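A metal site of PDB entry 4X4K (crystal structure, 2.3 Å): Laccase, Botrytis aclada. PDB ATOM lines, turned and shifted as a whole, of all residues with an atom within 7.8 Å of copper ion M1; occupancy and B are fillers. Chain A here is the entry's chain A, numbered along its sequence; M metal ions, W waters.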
ATOM      1  N   HIS A 124      19.981  -5.158  10.523  1.00  0.00           N
ATOM      2  CA  HIS A 124      20.348  -4.994  11.910  1.00  0.00           C
ATOM      3  C   HIS A 124      21.828  -4.655  12.108  1.00  0.00           C
ATOM      4  O   HIS A 124      22.717  -5.169  11.436  1.00  0.00           O
ATOM      5  CB  HIS A 124      19.954  -6.249  12.692  1.00  0.00           C
ATOM      6  CG  HIS A 124      20.465  -6.271  14.086  1.00  0.00           C
ATOM      7  ND1 HIS A 124      20.043  -5.386  15.047  1.00  0.00           N
ATOM      8  CD2 HIS A 124      21.359  -7.082  14.695  1.00  0.00           C
ATOM      9  CE1 HIS A 124      20.633  -5.653  16.195  1.00  0.00           C
ATOM     10  NE2 HIS A 124      21.452  -6.681  16.003  1.00  0.00           N
ATOM     11  N   TRP A 125      22.079  -3.757  13.059  1.00  0.00           N
ATOM     12  CA  TRP A 125      23.416  -3.266  13.380  1.00  0.00           C
ATOM     13  C   TRP A 125      23.790  -3.975  14.667  1.00  0.00           C
ATOM     14  O   TRP A 125      23.375  -3.588  15.760  1.00  0.00           O
ATOM     15  CB  TRP A 125      23.333  -1.743  13.475  1.00  0.00           C
ATOM     16  CG  TRP A 125      22.347  -1.280  12.401  1.00  0.00           C
ATOM     17  CD1 TRP A 125      21.019  -1.010  12.569  1.00  0.00           C
ATOM     18  CD2 TRP A 125      22.608  -1.125  11.007  1.00  0.00           C
ATOM     19  NE1 TRP A 125      20.443  -0.681  11.364  1.00  0.00           N
ATOM     20  CE2 TRP A 125      21.400  -0.747  10.391  1.00  0.00           C
ATOM     21  CE3 TRP A 125      23.764  -1.213  10.236  1.00  0.00           C
ATOM     22  CZ2 TRP A 125      21.303  -0.483   9.019  1.00  0.00           C
ATOM     23  CZ3 TRP A 125      23.656  -0.978   8.872  1.00  0.00           C
ATOM     24  CH2 TRP A 125      22.438  -0.599   8.286  1.00  0.00           C
ATOM     25  N   HIS A 126      24.553  -5.045  14.527  1.00  0.00           N
ATOM     26  CA  HIS A 126      24.717  -6.025  15.582  1.00  0.00           C
ATOM     27  C   HIS A 126      25.477  -5.465  16.757  1.00  0.00           C
ATOM     28  O   HIS A 126      26.583  -4.973  16.608  1.00  0.00           O
ATOM     29  CB  HIS A 126      25.405  -7.297  15.073  1.00  0.00           C
ATOM     30  CG  HIS A 126      25.608  -8.335  16.121  1.00  0.00           C
ATOM     31  ND1 HIS A 126      24.994  -9.561  16.080  1.00  0.00           N
ATOM     32  CD2 HIS A 126      26.324  -8.312  17.276  1.00  0.00           C
ATOM     33  CE1 HIS A 126      25.334 -10.260  17.153  1.00  0.00           C
ATOM     34  NE2 HIS A 126      26.142  -9.523  17.892  1.00  0.00           N
ATOM     35  N   GLY A 127      24.848  -5.536  17.928  1.00  0.00           N
ATOM     36  CA  GLY A 127      25.480  -5.094  19.172  1.00  0.00           C
ATOM     37  C   GLY A 127      25.331  -3.608  19.408  1.00  0.00           C
ATOM     38  O   GLY A 127      25.707  -3.107  20.483  1.00  0.00           O
ATOM     39  N   THR A 165      32.137  -4.519  15.085  1.00  0.00           N
ATOM     40  CA  THR A 165      30.960  -5.313  14.884  1.00  0.00           C
ATOM     41  C   THR A 165      30.657  -5.407  13.412  1.00  0.00           C
ATOM     42  O   THR A 165      31.536  -5.147  12.570  1.00  0.00           O
ATOM     43  CB  THR A 165      29.739  -4.816  15.723  1.00  0.00           C
ATOM     44  OG1 THR A 165      28.778  -5.863  15.771  1.00  0.00           O
ATOM     45  CG2 THR A 165      29.117  -3.559  15.146  1.00  0.00           C
ATOM     46  N   TRP A 166      29.408  -5.755  13.133  1.00  0.00           N
ATOM     47  CA  TRP A 166      28.955  -5.981  11.797  1.00  0.00           C
ATOM     48  C   TRP A 166      27.477  -5.621  11.695  1.00  0.00           C
ATOM     49  O   TRP A 166      26.775  -5.386  12.707  1.00  0.00           O
ATOM     50  CB  TRP A 166      29.208  -7.438  11.405  1.00  0.00           C
ATOM     51  CG  TRP A 166      28.571  -8.514  12.283  1.00  0.00           C
ATOM     52  CD1 TRP A 166      28.644  -8.628  13.650  1.00  0.00           C
ATOM     53  CD2 TRP A 166      27.814  -9.665  11.831  1.00  0.00           C
ATOM     54  NE1 TRP A 166      27.992  -9.764  14.064  1.00  0.00           N
ATOM     55  CE2 TRP A 166      27.467 -10.408  12.969  1.00  0.00           C
ATOM     56  CE3 TRP A 166      27.422 -10.131  10.575  1.00  0.00           C
ATOM     57  CZ2 TRP A 166      26.729 -11.575  12.901  1.00  0.00           C
ATOM     58  CZ3 TRP A 166      26.685 -11.271  10.495  1.00  0.00           C
ATOM     59  CH2 TRP A 166      26.354 -11.999  11.644  1.00  0.00           C
ATOM     60  N   TYR A 167      27.013  -5.538  10.454  1.00  0.00           N
ATOM     61  CA  TYR A 167      25.596  -5.355  10.163  1.00  0.00           C
ATOM     62  C   TYR A 167      25.173  -6.460   9.221  1.00  0.00           C
ATOM     63  O   TYR A 167      25.957  -6.929   8.409  1.00  0.00           O
ATOM     64  CB  TYR A 167      25.353  -3.982   9.533  1.00  0.00           C
ATOM     65  CG  TYR A 167      26.007  -3.750   8.178  1.00  0.00           C
ATOM     66  CD1 TYR A 167      27.361  -3.425   8.068  1.00  0.00           C
ATOM     67  CD2 TYR A 167      25.253  -3.796   7.017  1.00  0.00           C
ATOM     68  CE1 TYR A 167      27.942  -3.166   6.823  1.00  0.00           C
ATOM     69  CE2 TYR A 167      25.814  -3.568   5.778  1.00  0.00           C
ATOM     70  CZ  TYR A 167      27.164  -3.248   5.680  1.00  0.00           C
ATOM     71  OH  TYR A 167      27.698  -3.022   4.431  1.00  0.00           O
ATOM     72  N   HIS A 168      23.946  -6.915   9.342  1.00  0.00           N
ATOM     73  CA  HIS A 168      23.481  -8.003   8.516  1.00  0.00           C
ATOM     74  C   HIS A 168      21.976  -7.930   8.422  1.00  0.00           C
ATOM     75  O   HIS A 168      21.327  -7.315   9.259  1.00  0.00           O
ATOM     76  CB  HIS A 168      23.925  -9.345   9.107  1.00  0.00           C
ATOM     77  CG  HIS A 168      23.493  -9.590  10.531  1.00  0.00           C
ATOM     78  ND1 HIS A 168      22.231 -10.029  10.874  1.00  0.00           N
ATOM     79  CD2 HIS A 168      24.191  -9.519  11.694  1.00  0.00           C
ATOM     80  CE1 HIS A 168      22.162 -10.197  12.175  1.00  0.00           C
ATOM     81  NE2 HIS A 168      23.342  -9.897  12.701  1.00  0.00           N
ATOM     82  N   SER A 169      21.411  -8.570   7.413  1.00  0.00           N
ATOM     83  CA  SER A 169      19.959  -8.672   7.402  1.00  0.00           C
ATOM     84  C   SER A 169      19.489  -9.490   8.581  1.00  0.00           C
ATOM     85  O   SER A 169      20.171 -10.413   9.005  1.00  0.00           O
ATOM     86  CB  SER A 169      19.440  -9.320   6.138  1.00  0.00           C
ATOM     87  OG  SER A 169      18.118  -9.708   6.390  1.00  0.00           O
ATOM     88  N   HIS A 170      18.313  -9.152   9.089  1.00  0.00           N
ATOM     89  CA  HIS A 170      17.700  -9.918  10.145  1.00  0.00           C
ATOM     90  C   HIS A 170      16.430 -10.526   9.600  1.00  0.00           C
ATOM     91  O   HIS A 170      15.636 -11.078  10.344  1.00  0.00           O
ATOM     92  CB  HIS A 170      17.430  -9.075  11.390  1.00  0.00           C
ATOM     93  CG  HIS A 170      17.764  -9.775  12.669  1.00  0.00           C
ATOM     94  ND1 HIS A 170      17.191 -10.980  13.026  1.00  0.00           N
ATOM     95  CD2 HIS A 170      18.638  -9.472  13.651  1.00  0.00           C
ATOM     96  CE1 HIS A 170      17.697 -11.383  14.177  1.00  0.00           C
ATOM     97  NE2 HIS A 170      18.583 -10.485  14.578  1.00  0.00           N
ATOM     98  N   TYR A 175      21.240 -13.177   5.701  1.00  0.00           N
ATOM     99  CA  TYR A 175      22.693 -12.996   5.934  1.00  0.00           C
ATOM    100  C   TYR A 175      23.512 -14.212   5.521  1.00  0.00           C
ATOM    101  O   TYR A 175      24.705 -14.086   5.226  1.00  0.00           O
ATOM    102  CB  TYR A 175      23.042 -12.501   7.335  1.00  0.00           C
ATOM    103  CG  TYR A 175      23.254 -13.536   8.420  1.00  0.00           C
ATOM    104  CD1 TYR A 175      24.469 -14.172   8.537  1.00  0.00           C
ATOM    105  CD2 TYR A 175      22.254 -13.812   9.372  1.00  0.00           C
ATOM    106  CE1 TYR A 175      24.689 -15.092   9.531  1.00  0.00           C
ATOM    107  CE2 TYR A 175      22.467 -14.744  10.391  1.00  0.00           C
ATOM    108  CZ  TYR A 175      23.702 -15.392  10.452  1.00  0.00           C
ATOM    109  OH  TYR A 175      23.986 -16.336  11.423  1.00  0.00           O
ATOM    110  N   ASN A 269      32.808 -14.068  13.578  1.00  0.00           N
ATOM    111  CA  ASN A 269      32.241 -15.297  13.060  1.00  0.00           C
ATOM    112  C   ASN A 269      30.832 -14.927  12.565  1.00  0.00           C
ATOM    113  O   ASN A 269      29.957 -14.480  13.340  1.00  0.00           O
ATOM    114  CB  ASN A 269      32.252 -16.404  14.133  1.00  0.00           C
ATOM    115  CG  ASN A 269      31.507 -17.663  13.709  1.00  0.00           C
ATOM    116  OD1 ASN A 269      30.913 -17.761  12.621  1.00  0.00           O
ATOM    117  ND2 ASN A 269      31.526 -18.661  14.600  1.00  0.00           N
ATOM    118  N   VAL A 270      30.630 -15.098  11.257  1.00  0.00           N
ATOM    119  CA  VAL A 270      29.402 -14.693  10.598  1.00  0.00           C
ATOM    120  C   VAL A 270      28.736 -15.868   9.858  1.00  0.00           C
ATOM    121  O   VAL A 270      27.899 -15.673   8.990  1.00  0.00           O
ATOM    122  CB  VAL A 270      29.589 -13.474   9.659  1.00  0.00           C
ATOM    123  CG1 VAL A 270      30.008 -12.246  10.453  1.00  0.00           C
ATOM    124  CG2 VAL A 270      30.562 -13.760   8.519  1.00  0.00           C
ATOM    125  N   ILE A 307      29.062 -17.719  16.729  1.00  0.00           N
ATOM    126  CA  ILE A 307      28.497 -16.925  15.632  1.00  0.00           C
ATOM    127  C   ILE A 307      28.047 -15.585  16.170  1.00  0.00           C
ATOM    128  O   ILE A 307      27.329 -15.541  17.164  1.00  0.00           O
ATOM    129  CB  ILE A 307      27.288 -17.589  14.927  1.00  0.00           C
ATOM    130  CG1 ILE A 307      27.685 -18.903  14.288  1.00  0.00           C
ATOM    131  CG2 ILE A 307      26.729 -16.643  13.859  1.00  0.00           C
ATOM    132  CD1 ILE A 307      26.499 -19.605  13.653  1.00  0.00           C
ATOM    133  N   GLY A 308      28.461 -14.520  15.510  1.00  0.00           N
ATOM    134  CA  GLY A 308      28.068 -13.165  15.879  1.00  0.00           C
ATOM    135  C   GLY A 308      28.973 -12.545  16.924  1.00  0.00           C
ATOM    136  O   GLY A 308      28.869 -11.354  17.210  1.00  0.00           O
ATOM    137  N   GLN A 309      29.856 -13.347  17.502  1.00  0.00           N
ATOM    138  CA  GLN A 309      30.893 -12.843  18.382  1.00  0.00           C
ATOM    139  C   GLN A 309      31.996 -12.148  17.592  1.00  0.00           C
ATOM    140  O   GLN A 309      32.245 -12.487  16.414  1.00  0.00           O
ATOM    141  CB  GLN A 309      31.503 -13.979  19.203  1.00  0.00           C
ATOM    142  CG  GLN A 309      30.601 -14.476  20.309  1.00  0.00           C
ATOM    143  CD  GLN A 309      31.284 -15.429  21.265  1.00  0.00           C
ATOM    144  OE1 GLN A 309      32.122 -16.233  20.858  1.00  0.00           O
ATOM    145  NE2 GLN A 309      30.935 -15.331  22.530  1.00  0.00           N
ATOM    146  N   ARG A 310      32.641 -11.174  18.236  1.00  0.00           N
ATOM    147  CA  ARG A 310      33.811 -10.498  17.723  1.00  0.00           C
ATOM    148  C   ARG A 310      34.932 -10.545  18.741  1.00  0.00           C
ATOM    149  O   ARG A 310      34.688 -10.473  19.954  1.00  0.00           O
ATOM    150  CB  ARG A 310      33.535  -9.030  17.375  1.00  0.00           C
ATOM    151  CG  ARG A 310      32.571  -8.866  16.206  1.00  0.00           C
ATOM    152  CD  ARG A 310      31.120  -8.973  16.657  1.00  0.00           C
ATOM    153  NE  ARG A 310      30.707  -7.822  17.451  1.00  0.00           N
ATOM    154  CZ  ARG A 310      29.752  -7.848  18.384  1.00  0.00           C
ATOM    155  NH1 ARG A 310      29.126  -8.975  18.688  1.00  0.00           N
ATOM    156  NH2 ARG A 310      29.448  -6.739  19.030  1.00  0.00           N
ATOM    157  N   HIS A 466      22.396 -14.256  21.490  1.00  0.00           N
ATOM    158  CA  HIS A 466      22.565 -12.847  21.224  1.00  0.00           C
ATOM    159  C   HIS A 466      21.431 -11.997  21.797  1.00  0.00           C
ATOM    160  O   HIS A 466      20.281 -12.236  21.476  1.00  0.00           O
ATOM    161  CB  HIS A 466      22.684 -12.600  19.724  1.00  0.00           C
ATOM    162  CG  HIS A 466      22.794 -11.149  19.371  1.00  0.00           C
ATOM    163  ND1 HIS A 466      23.583 -10.278  20.092  1.00  0.00           N
ATOM    164  CD2 HIS A 466      22.172 -10.409  18.425  1.00  0.00           C
ATOM    165  CE1 HIS A 466      23.461  -9.064  19.588  1.00  0.00           C
ATOM    166  NE2 HIS A 466      22.616  -9.123  18.571  1.00  0.00           N
ATOM    167  N   HIS A 468      19.734  -8.234  21.933  1.00  0.00           N
ATOM    168  CA  HIS A 468      19.609  -6.894  21.340  1.00  0.00           C
ATOM    169  C   HIS A 468      19.420  -5.824  22.405  1.00  0.00           C
ATOM    170  O   HIS A 468      18.912  -6.112  23.506  1.00  0.00           O
ATOM    171  CB  HIS A 468      18.436  -6.833  20.376  1.00  0.00           C
ATOM    172  CG  HIS A 468      18.641  -7.616  19.115  1.00  0.00           C
ATOM    173  ND1 HIS A 468      18.432  -7.082  17.863  1.00  0.00           N
ATOM    174  CD2 HIS A 468      19.003  -8.902  18.912  1.00  0.00           C
ATOM    175  CE1 HIS A 468      18.684  -7.989  16.938  1.00  0.00           C
ATOM    176  NE2 HIS A 468      19.017  -9.106  17.540  1.00  0.00           N
ATOM    177  N   ASP A 500      27.856  -9.173  23.930  1.00  0.00           N
ATOM    178  CA  ASP A 500      26.470  -9.275  23.448  1.00  0.00           C
ATOM    179  C   ASP A 500      26.096 -10.598  22.768  1.00  0.00           C
ATOM    180  O   ASP A 500      24.930 -10.843  22.432  1.00  0.00           O
ATOM    181  CB  ASP A 500      26.104  -8.052  22.569  1.00  0.00           C
ATOM    182  CG  ASP A 500      26.885  -7.997  21.269  1.00  0.00           C
ATOM    183  OD1 ASP A 500      26.789  -8.966  20.478  1.00  0.00           O
ATOM    184  OD2 ASP A 500      27.573  -6.983  21.037  1.00  0.00           O
ATOM    185  N   VAL A 501      27.104 -11.454  22.564  1.00  0.00           N
ATOM    186  CA  VAL A 501      26.907 -12.862  22.196  1.00  0.00           C
ATOM    187  C   VAL A 501      27.677 -13.742  23.155  1.00  0.00           C
ATOM    188  O   VAL A 501      28.863 -13.512  23.378  1.00  0.00           O
ATOM    189  CB  VAL A 501      27.320 -13.178  20.749  1.00  0.00           C
ATOM    190  CG1 VAL A 501      27.083 -14.642  20.424  1.00  0.00           C
ATOM    191  CG2 VAL A 501      26.521 -12.319  19.788  1.00  0.00           C
ATOM    192  N   HIS A 525      18.104 -14.238  20.928  1.00  0.00           N
ATOM    193  CA  HIS A 525      17.961 -15.390  20.080  1.00  0.00           C
ATOM    194  C   HIS A 525      19.252 -16.142  19.919  1.00  0.00           C
ATOM    195  O   HIS A 525      20.355 -15.607  20.165  1.00  0.00           O
ATOM    196  CB  HIS A 525      17.402 -14.978  18.709  1.00  0.00           C
ATOM    197  CG  HIS A 525      18.304 -14.060  17.944  1.00  0.00           C
ATOM    198  ND1 HIS A 525      19.182 -14.520  16.979  1.00  0.00           N
ATOM    199  CD2 HIS A 525      18.498 -12.724  18.029  1.00  0.00           C
ATOM    200  CE1 HIS A 525      19.868 -13.489  16.497  1.00  0.00           C
ATOM    201  NE2 HIS A 525      19.469 -12.400  17.115  1.00  0.00           N
ATOM    202  N   HIS A 527      22.010 -17.229  17.596  1.00  0.00           N
ATOM    203  CA  HIS A 527      22.533 -16.649  16.365  1.00  0.00           C
ATOM    204  C   HIS A 527      22.873 -17.659  15.276  1.00  0.00           C
ATOM    205  O   HIS A 527      23.335 -17.278  14.187  1.00  0.00           O
ATOM    206  CB  HIS A 527      23.724 -15.726  16.643  1.00  0.00           C
ATOM    207  CG  HIS A 527      23.731 -14.487  15.787  1.00  0.00           C
ATOM    208  ND1 HIS A 527      23.753 -14.533  14.408  1.00  0.00           N
ATOM    209  CD2 HIS A 527      23.724 -13.170  16.125  1.00  0.00           C
ATOM    210  CE1 HIS A 527      23.748 -13.301  13.930  1.00  0.00           C
ATOM    211  NE2 HIS A 527      23.748 -12.454  14.944  1.00  0.00           N
HETATM  212 CU    CU M   1      23.899 -10.397  14.569  1.00  0.00          CU
HETATM  213 CU    CU M   2      22.051  -7.932  17.387  1.00  0.00          CU
HETATM  214 CU    CU M   3      19.508 -10.615  16.408  1.00  0.00          CU
HETATM  215  O   HOH W   1      21.333 -10.654  15.529  1.00  0.00           O
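The backbone NH (N) of His 124 is in hydrogen-bond range of the backbone carbonyl oxygen (O) of His 168, at 2.8 Å.
N of His 126 lies within hydrogen-bond range of O of Trp 166 (2.9 Å).
NE2 of His 126 sits close to ND1 of His 466.
A ring nitrogen (NE2) of His 126 lies within hydrogen-bond range of the backbone carbonyl oxygen of Gly 308 (3.4 Å).
The side-chain carboxylate (OD1) of Asp 500 is in hydrogen-bond range of a ring nitrogen (NE2) of His 126.
OG1 of Thr 165 is in hydrogen-bond range of O of His 126, at 2.5 Å.
NH1 of Arg 310 lies within hydrogen-bond range of NE2 of His 126 (3.1 Å).
OH of Tyr 175 sits at hydrogen-bond distance from O of His 527, 3.0 Å away.
Trp 166 touches copper ion M1.
Copper ion M1 is bound by NE2 of His 168, ND1 of His 126 and NE2 of His 527.
Slightly farther from copper ion M1 lies water W1 (2.8 Å).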
